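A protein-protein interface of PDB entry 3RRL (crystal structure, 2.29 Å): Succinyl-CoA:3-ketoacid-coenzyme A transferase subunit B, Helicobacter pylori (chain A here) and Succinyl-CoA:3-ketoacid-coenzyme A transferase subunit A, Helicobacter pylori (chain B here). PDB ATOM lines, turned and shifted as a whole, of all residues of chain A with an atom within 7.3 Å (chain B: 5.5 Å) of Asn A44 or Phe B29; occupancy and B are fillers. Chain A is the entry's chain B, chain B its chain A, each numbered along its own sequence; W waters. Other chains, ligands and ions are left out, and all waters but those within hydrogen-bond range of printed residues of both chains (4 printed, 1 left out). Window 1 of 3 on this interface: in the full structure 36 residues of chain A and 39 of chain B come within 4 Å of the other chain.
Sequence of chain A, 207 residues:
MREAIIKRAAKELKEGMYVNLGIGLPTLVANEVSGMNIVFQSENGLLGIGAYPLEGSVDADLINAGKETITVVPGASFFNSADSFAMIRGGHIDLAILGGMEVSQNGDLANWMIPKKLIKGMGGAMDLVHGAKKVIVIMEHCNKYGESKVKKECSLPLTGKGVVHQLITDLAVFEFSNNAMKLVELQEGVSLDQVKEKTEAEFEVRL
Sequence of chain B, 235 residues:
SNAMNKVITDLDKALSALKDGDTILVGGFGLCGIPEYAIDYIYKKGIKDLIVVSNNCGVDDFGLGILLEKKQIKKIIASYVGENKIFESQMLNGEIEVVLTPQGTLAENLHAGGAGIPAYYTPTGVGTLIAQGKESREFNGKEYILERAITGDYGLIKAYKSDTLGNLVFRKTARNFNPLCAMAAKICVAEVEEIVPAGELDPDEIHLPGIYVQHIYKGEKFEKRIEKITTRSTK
SG of Cys B32 sits at hydrogen-bond distance from O of Ala A60 (3.7 Å). SG of Cys B32 sits at hydrogen-bond distance from O of Asp A61. The backbone carbonyl oxygen of Asp A61 lies within hydrogen-bond range of the side-chain hydroxyl of Thr B173 (2.8 Å). OG1 of Thr B173 lies within hydrogen-bond range of N of Ile A63 (3.1 Å). O of Asn B176 sits at hydrogen-bond distance from N of Ser A81 (3.0 Å). OG of Ser A81 sits close to N of Phe B177, 3.4 Å away.
CG of Glu A43 touches OE1 of Gln B103, 3.9 Å away. Phe B29 touches Asn A44. Asn A44 touches Thr B173. Leu A46 touches Thr B173. CA of Leu A62 touches OG1 of Thr B173, at 3.6 Å. CD1 of Ile A63 touches CD1 of Phe B29, 3.95 Å away. CD1 of Ile A63 touches CB of Cys B32, at 3.6 Å. NZ of Lys A67 touches CE1 of Phe B29, 3.2 Å away. CA of Gly B30 touches CE of Lys A67, at 3.9 Å. Thr B173 touches Phe A78.
Gln A41 touches none of the printed residues of chain B. Of the printed residues of chain A, Phe B29 touches Asn A44 (3.8 Å), Ile A63 (3.95 Å), Asn A64 (3.998 Å), Ala A65 (3.6 Å) and Lys A67 (3.2 Å). Printed residues of chain A within 4 Å of Cys B32: Ala A60 (3.7 Å), Asp A61 (3.5 Å) and Ile A63 (3.6 Å). Printed residues of chain A within 4 Å of Asn B176: Asn A80 (3.3 Å) and Ser A81 (3.0 Å). The nearest residue of chain B that does not touch Asn A44 is Asn B176 (4.04 Å). The nearest printed residue of chain A that does not touch Phe B29 is Glu A43 (4.8 Å).
Of the 14 printed residues of chain B, 7 touch a printed residue of chain A. Printed residues of chain B that touch a printed residue of chain A: Phe B29, Gly B30, Cys B32, Gln B103, Thr B173, Asn B176 and Phe B177. Hydrophobic or aromatic side chains of chain B within 4 Å of the printed part of chain A: Phe B29 and Phe B177. Hydrophobic or aromatic side chains of chain A within 4 Å of the printed part of chain B: Leu A46, Leu A62, Ile A63, Phe A78 and Phe A85. Among the printed residues, no Asp or Glu carboxylate lies within 4 Å of a Lys or Arg side-chain nitrogen of the other chain.
The side-chain amide nitrogen of Asn B176 sits close to the backbone NH of Phe B29 (3.4 Å). The backbone carbonyl oxygen (O) of Cys B32 sits at hydrogen-bond distance from the side-chain amide nitrogen (ND2) of Asn B176 (3.1 Å). O of Ile A63 is in hydrogen-bond range of ND2 of Asn A44 (2.9 Å). The backbone NH (N) of Gly A66 sits at hydrogen-bond distance from the side-chain amide oxygen (OD1) of Asn A64 (2.9 Å).
Water W2 lies within hydrogen-bond range of the backbone carbonyl oxygen (O) of Glu A43 (2.5 Å), the side-chain hydroxyl (OG) of Ser A81 (2.7 Å) and the side-chain amide oxygen (OE1) of Gln B103 (3.1 Å). Water W4 bridges the side-chain carboxylate (OD1) of Asp A61 (2.6 Å) and the backbone NH (N) of Gly B33 (3.4 Å). Water W1 lies within hydrogen-bond range of O of Thr B173 (2.8 Å), ND2 of Asn A44 (2.9 Å) and SG of Cys B32 (3.2 Å).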
ATOM      1  N   ASN A  20       2.231  13.595  -3.095  1.00  0.00           N
ATOM      2  CA  ASN A  20       1.930  14.555  -4.142  1.00  0.00           C
ATOM      3  C   ASN A  20       2.356  14.041  -5.511  1.00  0.00           C
ATOM      4  O   ASN A  20       3.524  13.708  -5.725  1.00  0.00           O
ATOM      5  CB  ASN A  20       2.595  15.895  -3.869  1.00  0.00           C
ATOM      6  CG  ASN A  20       2.256  16.921  -4.928  1.00  0.00           C
ATOM      7  OD1 ASN A  20       2.699  16.818  -6.080  1.00  0.00           O
ATOM      8  ND2 ASN A  20       1.447  17.914  -4.551  1.00  0.00           N
ATOM      9  N   GLN A  41      -2.185  15.010  -1.988  1.00  0.00           N
ATOM     10  CA  GLN A  41      -2.204  16.447  -1.779  1.00  0.00           C
ATOM     11  C   GLN A  41      -2.209  17.159  -3.123  1.00  0.00           C
ATOM     12  O   GLN A  41      -1.509  16.752  -4.043  1.00  0.00           O
ATOM     13  CB  GLN A  41      -0.977  16.871  -0.971  1.00  0.00           C
ATOM     14  CG  GLN A  41      -1.077  18.252  -0.335  1.00  0.00           C
ATOM     15  CD  GLN A  41      -0.358  19.323  -1.122  1.00  0.00           C
ATOM     16  OE1 GLN A  41      -0.040  19.138  -2.299  1.00  0.00           O
ATOM     17  NE2 GLN A  41      -0.099  20.461  -0.476  1.00  0.00           N
ATOM     18  N   SER A  42      -3.010  18.212  -3.237  1.00  0.00           N
ATOM     19  CA  SER A  42      -3.028  19.022  -4.447  1.00  0.00           C
ATOM     20  C   SER A  42      -2.478  20.381  -4.060  1.00  0.00           C
ATOM     21  O   SER A  42      -2.920  20.974  -3.071  1.00  0.00           O
ATOM     22  CB  SER A  42      -4.453  19.143  -4.991  1.00  0.00           C
ATOM     23  OG  SER A  42      -4.465  19.600  -6.333  1.00  0.00           O
ATOM     24  N   GLU A  43      -1.498  20.865  -4.817  1.00  0.00           N
ATOM     25  CA  GLU A  43      -0.730  22.043  -4.408  1.00  0.00           C
ATOM     26  C   GLU A  43      -1.561  23.326  -4.423  1.00  0.00           C
ATOM     27  O   GLU A  43      -1.144  24.363  -3.902  1.00  0.00           O
ATOM     28  CB  GLU A  43       0.504  22.203  -5.295  1.00  0.00           C
ATOM     29  CG  GLU A  43       0.179  22.521  -6.733  1.00  0.00           C
ATOM     30  CD  GLU A  43       1.200  21.952  -7.700  1.00  0.00           C
ATOM     31  OE1 GLU A  43       2.063  21.168  -7.252  1.00  0.00           O
ATOM     32  OE2 GLU A  43       1.139  22.287  -8.903  1.00  0.00           O
ATOM     33  N   ASN A  44      -2.752  23.233  -5.001  1.00  0.00           N
ATOM     34  CA  ASN A  44      -3.638  24.376  -5.133  1.00  0.00           C
ATOM     35  C   ASN A  44      -4.505  24.553  -3.889  1.00  0.00           C
ATOM     36  O   ASN A  44      -5.442  25.357  -3.875  1.00  0.00           O
ATOM     37  CB  ASN A  44      -4.451  24.347  -6.430  1.00  0.00           C
ATOM     38  CG  ASN A  44      -5.221  23.062  -6.617  1.00  0.00           C
ATOM     39  OD1 ASN A  44      -4.737  21.977  -6.307  1.00  0.00           O
ATOM     40  ND2 ASN A  44      -6.429  23.178  -7.151  1.00  0.00           N
ATOM     41  N   GLY A  45      -4.165  23.818  -2.832  1.00  0.00           N
ATOM     42  CA  GLY A  45      -4.852  23.990  -1.564  1.00  0.00           C
ATOM     43  C   GLY A  45      -5.817  22.926  -1.090  1.00  0.00           C
ATOM     44  O   GLY A  45      -6.775  23.219  -0.382  1.00  0.00           O
ATOM     45  N   LEU A  46      -5.609  21.694  -1.522  1.00  0.00           N
ATOM     46  CA  LEU A  46      -6.398  20.601  -0.989  1.00  0.00           C
ATOM     47  C   LEU A  46      -5.550  19.451  -0.463  1.00  0.00           C
ATOM     48  O   LEU A  46      -4.520  19.097  -1.042  1.00  0.00           O
ATOM     49  CB  LEU A  46      -7.362  20.089  -2.049  1.00  0.00           C
ATOM     50  CG  LEU A  46      -7.834  18.650  -1.866  1.00  0.00           C
ATOM     51  CD1 LEU A  46      -8.835  18.552  -0.710  1.00  0.00           C
ATOM     52  CD2 LEU A  46      -8.449  18.172  -3.183  1.00  0.00           C
ATOM     53  N   ILE A  49      -7.361  14.482  -2.098  1.00  0.00           N
ATOM     54  CA  ILE A  49      -7.886  14.301  -3.452  1.00  0.00           C
ATOM     55  C   ILE A  49      -8.676  12.990  -3.599  1.00  0.00           C
ATOM     56  O   ILE A  49      -8.349  11.972  -2.982  1.00  0.00           O
ATOM     57  CB  ILE A  49      -6.754  14.263  -4.497  1.00  0.00           C
ATOM     58  CG1 ILE A  49      -5.973  15.570  -4.519  1.00  0.00           C
ATOM     59  CG2 ILE A  49      -7.299  13.961  -5.900  1.00  0.00           C
ATOM     60  CD1 ILE A  49      -4.824  15.533  -5.518  1.00  0.00           C
ATOM     61  N   ALA A  60     -16.821  23.611 -10.546  1.00  0.00           N
ATOM     62  CA  ALA A  60     -15.705  24.377 -11.096  1.00  0.00           C
ATOM     63  C   ALA A  60     -14.738  24.845 -10.014  1.00  0.00           C
ATOM     64  O   ALA A  60     -13.548  25.031 -10.276  1.00  0.00           O
ATOM     65  CB  ALA A  60     -16.225  25.574 -11.875  1.00  0.00           C
ATOM     66  N   ASP A  61     -15.249  25.056  -8.804  1.00  0.00           N
ATOM     67  CA  ASP A  61     -14.411  25.517  -7.701  1.00  0.00           C
ATOM     68  C   ASP A  61     -13.513  24.404  -7.162  1.00  0.00           C
ATOM     69  O   ASP A  61     -12.662  24.644  -6.307  1.00  0.00           O
ATOM     70  CB  ASP A  61     -15.268  26.080  -6.560  1.00  0.00           C
ATOM     71  CG  ASP A  61     -15.862  27.443  -6.886  1.00  0.00           C
ATOM     72  OD1 ASP A  61     -15.330  28.140  -7.776  1.00  0.00           O
ATOM     73  OD2 ASP A  61     -16.861  27.823  -6.241  1.00  0.00           O
ATOM     74  N   LEU A  62     -13.714  23.181  -7.636  1.00  0.00           N
ATOM     75  CA  LEU A  62     -12.915  22.074  -7.133  1.00  0.00           C
ATOM     76  C   LEU A  62     -12.129  21.367  -8.238  1.00  0.00           C
ATOM     77  O   LEU A  62     -12.686  20.596  -9.022  1.00  0.00           O
ATOM     78  CB  LEU A  62     -13.834  21.091  -6.405  1.00  0.00           C
ATOM     79  CG  LEU A  62     -13.220  19.835  -5.797  1.00  0.00           C
ATOM     80  CD1 LEU A  62     -12.066  20.194  -4.874  1.00  0.00           C
ATOM     81  CD2 LEU A  62     -14.304  19.046  -5.061  1.00  0.00           C
ATOM     82  N   ILE A  63     -10.818  21.583  -8.255  1.00  0.00           N
ATOM     83  CA  ILE A  63      -9.964  21.022  -9.300  1.00  0.00           C
ATOM     84  C   ILE A  63      -8.624  20.558  -8.749  1.00  0.00           C
ATOM     85  O   ILE A  63      -8.236  20.919  -7.643  1.00  0.00           O
ATOM     86  CB  ILE A  63      -9.692  22.039 -10.423  1.00  0.00           C
ATOM     87  CG1 ILE A  63      -9.071  23.312  -9.841  1.00  0.00           C
ATOM     88  CG2 ILE A  63     -10.980  22.350 -11.181  1.00  0.00           C
ATOM     89  CD1 ILE A  63      -8.488  24.244 -10.879  1.00  0.00           C
ATOM     90  N   ASN A  64      -7.920  19.746  -9.525  1.00  0.00           N
ATOM     91  CA  ASN A  64      -6.576  19.344  -9.155  1.00  0.00           C
ATOM     92  C   ASN A  64      -5.581  20.290  -9.807  1.00  0.00           C
ATOM     93  O   ASN A  64      -5.975  21.241 -10.484  1.00  0.00           O
ATOM     94  CB  ASN A  64      -6.307  17.888  -9.553  1.00  0.00           C
ATOM     95  CG  ASN A  64      -6.417  17.647 -11.058  1.00  0.00           C
ATOM     96  OD1 ASN A  64      -6.375  18.582 -11.866  1.00  0.00           O
ATOM     97  ND2 ASN A  64      -6.554  16.380 -11.437  1.00  0.00           N
ATOM     98  N   ALA A  65      -4.295  20.036  -9.609  1.00  0.00           N
ATOM     99  CA  ALA A  65      -3.274  20.940 -10.114  1.00  0.00           C
ATOM    100  C   ALA A  65      -3.366  21.040 -11.622  1.00  0.00           C
ATOM    101  O   ALA A  65      -2.934  22.034 -12.209  1.00  0.00           O
ATOM    102  CB  ALA A  65      -1.896  20.466  -9.702  1.00  0.00           C
ATOM    103  N   GLY A  66      -3.929  20.002 -12.242  1.00  0.00           N
ATOM    104  CA  GLY A  66      -4.027  19.928 -13.688  1.00  0.00           C
ATOM    105  C   GLY A  66      -5.280  20.592 -14.232  1.00  0.00           C
ATOM    106  O   GLY A  66      -5.625  20.404 -15.394  1.00  0.00           O
ATOM    107  N   LYS A  67      -5.958  21.368 -13.389  1.00  0.00           N
ATOM    108  CA  LYS A  67      -7.181  22.078 -13.779  1.00  0.00           C
ATOM    109  C   LYS A  67      -8.316  21.124 -14.162  1.00  0.00           C
ATOM    110  O   LYS A  67      -9.212  21.486 -14.928  1.00  0.00           O
ATOM    111  CB  LYS A  67      -6.917  23.068 -14.924  1.00  0.00           C
ATOM    112  CG  LYS A  67      -5.599  23.826 -14.819  1.00  0.00           C
ATOM    113  CD  LYS A  67      -5.478  24.578 -13.501  1.00  0.00           C
ATOM    114  CE  LYS A  67      -4.190  25.400 -13.431  1.00  0.00           C
ATOM    115  NZ  LYS A  67      -2.958  24.568 -13.254  1.00  0.00           N
ATOM    116  N   GLU A  68      -8.278  19.912 -13.618  1.00  0.00           N
ATOM    117  CA  GLU A  68      -9.339  18.934 -13.839  1.00  0.00           C
ATOM    118  C   GLU A  68     -10.339  18.955 -12.689  1.00  0.00           C
ATOM    119  O   GLU A  68      -9.962  19.153 -11.530  1.00  0.00           O
ATOM    120  CB  GLU A  68      -8.749  17.534 -13.965  1.00  0.00           C
ATOM    121  CG  GLU A  68      -7.671  17.415 -15.027  1.00  0.00           C
ATOM    122  CD  GLU A  68      -7.116  16.003 -15.137  1.00  0.00           C
ATOM    123  OE1 GLU A  68      -7.078  15.295 -14.105  1.00  0.00           O
ATOM    124  OE2 GLU A  68      -6.721  15.601 -16.257  1.00  0.00           O
ATOM    125  N   ILE A  70     -12.580  17.485  -9.868  1.00  0.00           N
ATOM    126  CA  ILE A  70     -12.410  16.313  -9.005  1.00  0.00           C
ATOM    127  C   ILE A  70     -13.402  16.306  -7.853  1.00  0.00           C
ATOM    128  O   ILE A  70     -14.275  17.165  -7.768  1.00  0.00           O
ATOM    129  CB  ILE A  70     -10.994  16.260  -8.399  1.00  0.00           C
ATOM    130  CG1 ILE A  70     -10.703  17.550  -7.631  1.00  0.00           C
ATOM    131  CG2 ILE A  70      -9.957  16.049  -9.488  1.00  0.00           C
ATOM    132  CD1 ILE A  70      -9.406  17.503  -6.817  1.00  0.00           C
ATOM    133  N   PHE A  78      -9.239  21.989   2.948  1.00  0.00           N
ATOM    134  CA  PHE A  78      -8.830  22.999   1.986  1.00  0.00           C
ATOM    135  C   PHE A  78      -8.008  24.041   2.717  1.00  0.00           C
ATOM    136  O   PHE A  78      -8.191  24.263   3.918  1.00  0.00           O
ATOM    137  CB  PHE A  78     -10.039  23.670   1.319  1.00  0.00           C
ATOM    138  CG  PHE A  78     -10.865  22.742   0.458  1.00  0.00           C
ATOM    139  CD1 PHE A  78     -10.344  22.201  -0.698  1.00  0.00           C
ATOM    140  CD2 PHE A  78     -12.175  22.441   0.792  1.00  0.00           C
ATOM    141  CE1 PHE A  78     -11.104  21.352  -1.490  1.00  0.00           C
ATOM    142  CE2 PHE A  78     -12.937  21.595   0.000  1.00  0.00           C
ATOM    143  CZ  PHE A  78     -12.397  21.045  -1.135  1.00  0.00           C
ATOM    144  N   PHE A  79      -7.086  24.671   1.996  1.00  0.00           N
ATOM    145  CA  PHE A  79      -6.279  25.732   2.573  1.00  0.00           C
ATOM    146  C   PHE A  79      -5.715  26.584   1.455  1.00  0.00           C
ATOM    147  O   PHE A  79      -5.875  26.252   0.276  1.00  0.00           O
ATOM    148  CB  PHE A  79      -5.149  25.127   3.410  1.00  0.00           C
ATOM    149  CG  PHE A  79      -4.620  23.843   2.852  1.00  0.00           C
ATOM    150  CD1 PHE A  79      -3.655  23.850   1.855  1.00  0.00           C
ATOM    151  CD2 PHE A  79      -5.094  22.625   3.313  1.00  0.00           C
ATOM    152  CE1 PHE A  79      -3.160  22.657   1.328  1.00  0.00           C
ATOM    153  CE2 PHE A  79      -4.604  21.424   2.796  1.00  0.00           C
ATOM    154  CZ  PHE A  79      -3.635  21.442   1.804  1.00  0.00           C
ATOM    155  N   ASN A  80      -5.036  27.668   1.823  1.00  0.00           N
ATOM    156  CA  ASN A  80      -4.555  28.613   0.824  1.00  0.00           C
ATOM    157  C   ASN A  80      -3.180  28.217   0.293  1.00  0.00           C
ATOM    158  O   ASN A  80      -2.591  27.220   0.737  1.00  0.00           O
ATOM    159  CB  ASN A  80      -4.614  30.072   1.328  1.00  0.00           C
ATOM    160  CG  ASN A  80      -3.522  30.409   2.341  1.00  0.00           C
ATOM    161  OD1 ASN A  80      -2.354  30.093   2.145  1.00  0.00           O
ATOM    162  ND2 ASN A  80      -3.908  31.070   3.424  1.00  0.00           N
ATOM    163  N   SER A  81      -2.680  28.988  -0.663  1.00  0.00           N
ATOM    164  CA  SER A  81      -1.505  28.571  -1.416  1.00  0.00           C
ATOM    165  C   SER A  81      -0.225  28.622  -0.595  1.00  0.00           C
ATOM    166  O   SER A  81       0.631  27.777  -0.766  1.00  0.00           O
ATOM    167  CB  SER A  81      -1.376  29.379  -2.703  1.00  0.00           C
ATOM    168  OG  SER A  81      -2.380  28.969  -3.619  1.00  0.00           O
ATOM    169  N   SER A  84      -0.354  25.529   1.626  1.00  0.00           N
ATOM    170  CA  SER A  84      -0.030  24.362   0.818  1.00  0.00           C
ATOM    171  C   SER A  84       1.473  24.213   0.707  1.00  0.00           C
ATOM    172  O   SER A  84       2.037  23.135   0.939  1.00  0.00           O
ATOM    173  CB  SER A  84      -0.612  24.516  -0.583  1.00  0.00           C
ATOM    174  OG  SER A  84      -0.342  23.369  -1.362  1.00  0.00           O
ATOM    175  N   PHE A  85       2.131  25.307   0.356  1.00  0.00           N
ATOM    176  CA  PHE A  85       3.561  25.249   0.135  1.00  0.00           C
ATOM    177  C   PHE A  85       4.361  25.265   1.438  1.00  0.00           C
ATOM    178  O   PHE A  85       5.502  24.815   1.468  1.00  0.00           O
ATOM    179  CB  PHE A  85       4.000  26.295  -0.895  1.00  0.00           C
ATOM    180  CG  PHE A  85       3.663  25.890  -2.305  1.00  0.00           C
ATOM    181  CD1 PHE A  85       4.408  24.915  -2.949  1.00  0.00           C
ATOM    182  CD2 PHE A  85       2.572  26.426  -2.958  1.00  0.00           C
ATOM    183  CE1 PHE A  85       4.085  24.503  -4.225  1.00  0.00           C
ATOM    184  CE2 PHE A  85       2.246  26.016  -4.239  1.00  0.00           C
ATOM    185  CZ  PHE A  85       3.008  25.052  -4.872  1.00  0.00           C
ATOM    186  N   ILE A  88       4.409  21.667   2.034  1.00  0.00           N
ATOM    187  CA  ILE A  88       5.382  21.056   1.137  1.00  0.00           C
ATOM    188  C   ILE A  88       6.819  21.416   1.516  1.00  0.00           C
ATOM    189  O   ILE A  88       7.663  20.537   1.681  1.00  0.00           O
ATOM    190  CB  ILE A  88       5.109  21.453  -0.317  1.00  0.00           C
ATOM    191  CG1 ILE A  88       3.883  20.697  -0.831  1.00  0.00           C
ATOM    192  CG2 ILE A  88       6.319  21.157  -1.187  1.00  0.00           C
ATOM    193  CD1 ILE A  88       3.287  21.263  -2.103  1.00  0.00           C
ATOM    194  N   GLY B  27      -6.017  37.119  -7.598  1.00  0.00           N
ATOM    195  CA  GLY B  27      -6.255  35.758  -7.158  1.00  0.00           C
ATOM    196  C   GLY B  27      -6.608  34.784  -8.273  1.00  0.00           C
ATOM    197  O   GLY B  27      -6.863  35.168  -9.418  1.00  0.00           O
ATOM    198  N   GLY B  28      -6.669  33.509  -7.905  1.00  0.00           N
ATOM    199  CA  GLY B  28      -7.076  32.442  -8.797  1.00  0.00           C
ATOM    200  C   GLY B  28      -5.970  31.485  -9.193  1.00  0.00           C
ATOM    201  O   GLY B  28      -4.795  31.843  -9.251  1.00  0.00           O
ATOM    202  N   PHE B  29      -6.381  30.251  -9.471  1.00  0.00           N
ATOM    203  CA  PHE B  29      -5.507  29.191  -9.945  1.00  0.00           C
ATOM    204  C   PHE B  29      -6.185  28.695 -11.210  1.00  0.00           C
ATOM    205  O   PHE B  29      -7.283  28.141 -11.151  1.00  0.00           O
ATOM    206  CB  PHE B  29      -5.452  28.071  -8.911  1.00  0.00           C
ATOM    207  CG  PHE B  29      -4.523  26.941  -9.268  1.00  0.00           C
ATOM    208  CD1 PHE B  29      -4.987  25.836  -9.968  1.00  0.00           C
ATOM    209  CD2 PHE B  29      -3.187  26.970  -8.874  1.00  0.00           C
ATOM    210  CE1 PHE B  29      -4.129  24.782 -10.289  1.00  0.00           C
ATOM    211  CE2 PHE B  29      -2.318  25.918  -9.189  1.00  0.00           C
ATOM    212  CZ  PHE B  29      -2.789  24.824  -9.900  1.00  0.00           C
ATOM    213  N   GLY B  30      -5.544  28.904 -12.352  1.00  0.00           N
ATOM    214  CA  GLY B  30      -6.205  28.710 -13.628  1.00  0.00           C
ATOM    215  C   GLY B  30      -7.388  29.658 -13.730  1.00  0.00           C
ATOM    216  O   GLY B  30      -7.246  30.876 -13.582  1.00  0.00           O
ATOM    217  N   LEU B  31      -8.555  29.092 -14.015  1.00  0.00           N
ATOM    218  CA  LEU B  31      -9.820  29.826 -14.022  1.00  0.00           C
ATOM    219  C   LEU B  31     -10.601  29.642 -12.719  1.00  0.00           C
ATOM    220  O   LEU B  31     -11.765  30.040 -12.620  1.00  0.00           O
ATOM    221  CB  LEU B  31     -10.668  29.422 -15.227  1.00  0.00           C
ATOM    222  CG  LEU B  31      -9.927  29.533 -16.561  1.00  0.00           C
ATOM    223  CD1 LEU B  31     -10.875  29.240 -17.721  1.00  0.00           C
ATOM    224  CD2 LEU B  31      -9.311  30.916 -16.703  1.00  0.00           C
ATOM    225  N   CYS B  32      -9.971  28.989 -11.746  1.00  0.00           N
ATOM    226  CA  CYS B  32     -10.622  28.656 -10.486  1.00  0.00           C
ATOM    227  C   CYS B  32     -10.378  29.733  -9.434  1.00  0.00           C
ATOM    228  O   CYS B  32      -9.248  29.946  -8.983  1.00  0.00           O
ATOM    229  CB  CYS B  32     -10.112  27.300  -9.992  1.00  0.00           C
ATOM    230  SG  CYS B  32     -10.828  26.701  -8.462  1.00  0.00           S
ATOM    231  N   GLY B  33     -11.445  30.417  -9.045  1.00  0.00           N
ATOM    232  CA  GLY B  33     -11.344  31.491  -8.071  1.00  0.00           C
ATOM    233  C   GLY B  33     -10.784  32.792  -8.625  1.00  0.00           C
ATOM    234  O   GLY B  33     -10.042  33.496  -7.938  1.00  0.00           O
ATOM    235  N   ILE B  34     -11.104  33.108  -9.876  1.00  0.00           N
ATOM    236  CA  ILE B  34     -10.654  34.367 -10.461  1.00  0.00           C
ATOM    237  C   ILE B  34     -11.683  35.489 -10.292  1.00  0.00           C
ATOM    238  O   ILE B  34     -12.887  35.234 -10.303  1.00  0.00           O
ATOM    239  CB  ILE B  34     -10.296  34.210 -11.948  1.00  0.00           C
ATOM    240  CG1 ILE B  34     -11.507  33.710 -12.742  1.00  0.00           C
ATOM    241  CG2 ILE B  34      -9.122  33.274 -12.109  1.00  0.00           C
ATOM    242  CD1 ILE B  34     -11.287  33.710 -14.243  1.00  0.00           C
ATOM    243  N   ASN B  55      -0.824  33.630 -10.183  1.00  0.00           N
ATOM    244  CA  ASN B  55      -0.200  32.328 -10.385  1.00  0.00           C
ATOM    245  C   ASN B  55      -0.097  31.971 -11.859  1.00  0.00           C
ATOM    246  O   ASN B  55       0.934  31.487 -12.324  1.00  0.00           O
ATOM    247  CB  ASN B  55      -0.961  31.226  -9.676  1.00  0.00           C
ATOM    248  CG  ASN B  55      -0.174  29.942  -9.635  1.00  0.00           C
ATOM    249  OD1 ASN B  55       0.988  29.945  -9.224  1.00  0.00           O
ATOM    250  ND2 ASN B  55      -0.783  28.843 -10.080  1.00  0.00           N
ATOM    251  N   ASN B  56      -1.194  32.191 -12.579  1.00  0.00           N
ATOM    252  CA  ASN B  56      -1.244  31.941 -14.007  1.00  0.00           C
ATOM    253  C   ASN B  56      -1.760  33.171 -14.739  1.00  0.00           C
ATOM    254  O   ASN B  56      -2.062  34.189 -14.119  1.00  0.00           O
ATOM    255  CB  ASN B  56      -2.132  30.729 -14.309  1.00  0.00           C
ATOM    256  CG  ASN B  56      -1.886  29.577 -13.355  1.00  0.00           C
ATOM    257  OD1 ASN B  56      -2.661  29.358 -12.425  1.00  0.00           O
ATOM    258  ND2 ASN B  56      -0.796  28.832 -13.578  1.00  0.00           N
ATOM    259  N   GLN B 103       6.019  28.497  -7.612  1.00  0.00           N
ATOM    260  CA  GLN B 103       4.694  28.741  -7.061  1.00  0.00           C
ATOM    261  C   GLN B 103       4.714  28.973  -5.541  1.00  0.00           C
ATOM    262  O   GLN B 103       4.048  29.872  -5.034  1.00  0.00           O
ATOM    263  CB  GLN B 103       3.761  27.585  -7.442  1.00  0.00           C
ATOM    264  CG  GLN B 103       2.302  27.806  -7.116  1.00  0.00           C
ATOM    265  CD  GLN B 103       1.417  26.790  -7.797  1.00  0.00           C
ATOM    266  OE1 GLN B 103       0.413  26.355  -7.243  1.00  0.00           O
ATOM    267  NE2 GLN B 103       1.784  26.409  -9.015  1.00  0.00           N
ATOM    268  N   THR B 173     -11.076  24.640  -3.731  1.00  0.00           N
ATOM    269  CA  THR B 173      -9.770  25.038  -4.235  1.00  0.00           C
ATOM    270  C   THR B 173      -9.810  26.397  -4.900  1.00  0.00           C
ATOM    271  O   THR B 173      -8.842  26.866  -5.437  1.00  0.00           O
ATOM    272  CB  THR B 173      -9.158  23.988  -5.166  1.00  0.00           C
ATOM    273  OG1 THR B 173      -9.940  23.858  -6.345  1.00  0.00           O
ATOM    274  CG2 THR B 173      -9.082  22.654  -4.472  1.00  0.00           C
ATOM    275  N   ASN B 176      -7.081  29.211  -3.043  1.00  0.00           N
ATOM    276  CA  ASN B 176      -5.747  29.436  -3.593  1.00  0.00           C
ATOM    277  C   ASN B 176      -4.979  30.660  -3.072  1.00  0.00           C
ATOM    278  O   ASN B 176      -4.705  30.790  -1.897  1.00  0.00           O
ATOM    279  CB  ASN B 176      -5.640  29.202  -5.105  1.00  0.00           C
ATOM    280  CG  ASN B 176      -6.545  30.082  -5.900  1.00  0.00           C
ATOM    281  OD1 ASN B 176      -6.256  31.240  -6.101  1.00  0.00           O
ATOM    282  ND2 ASN B 176      -7.638  29.529  -6.364  1.00  0.00           N
ATOM    283  N   PHE B 177      -4.637  31.534  -4.006  1.00  0.00           N
ATOM    284  CA  PHE B 177      -3.898  32.753  -3.756  1.00  0.00           C
ATOM    285  C   PHE B 177      -4.727  33.965  -3.324  1.00  0.00           C
ATOM    286  O   PHE B 177      -4.158  34.999  -3.018  1.00  0.00           O
ATOM    287  CB  PHE B 177      -3.127  33.136  -5.020  1.00  0.00           C
ATOM    288  CG  PHE B 177      -1.919  32.301  -5.269  1.00  0.00           C
ATOM    289  CD1 PHE B 177      -2.017  31.091  -5.909  1.00  0.00           C
ATOM    290  CD2 PHE B 177      -0.676  32.727  -4.865  1.00  0.00           C
ATOM    291  CE1 PHE B 177      -0.903  30.324  -6.125  1.00  0.00           C
ATOM    292  CE2 PHE B 177       0.429  31.960  -5.087  1.00  0.00           C
ATOM    293  CZ  PHE B 177       0.315  30.761  -5.716  1.00  0.00           C
HETATM  294  O   HOH W   1      -7.900  25.568  -7.676  1.00  0.00           O
HETATM  295  O   HOH W   2      -1.406  26.734  -4.745  1.00  0.00           O
HETATM  296  O   HOH W   3      -7.229  26.572  -2.215  1.00  0.00           O
HETATM  297  O   HOH W   4     -14.186  28.750 -10.076  1.00  0.00           O
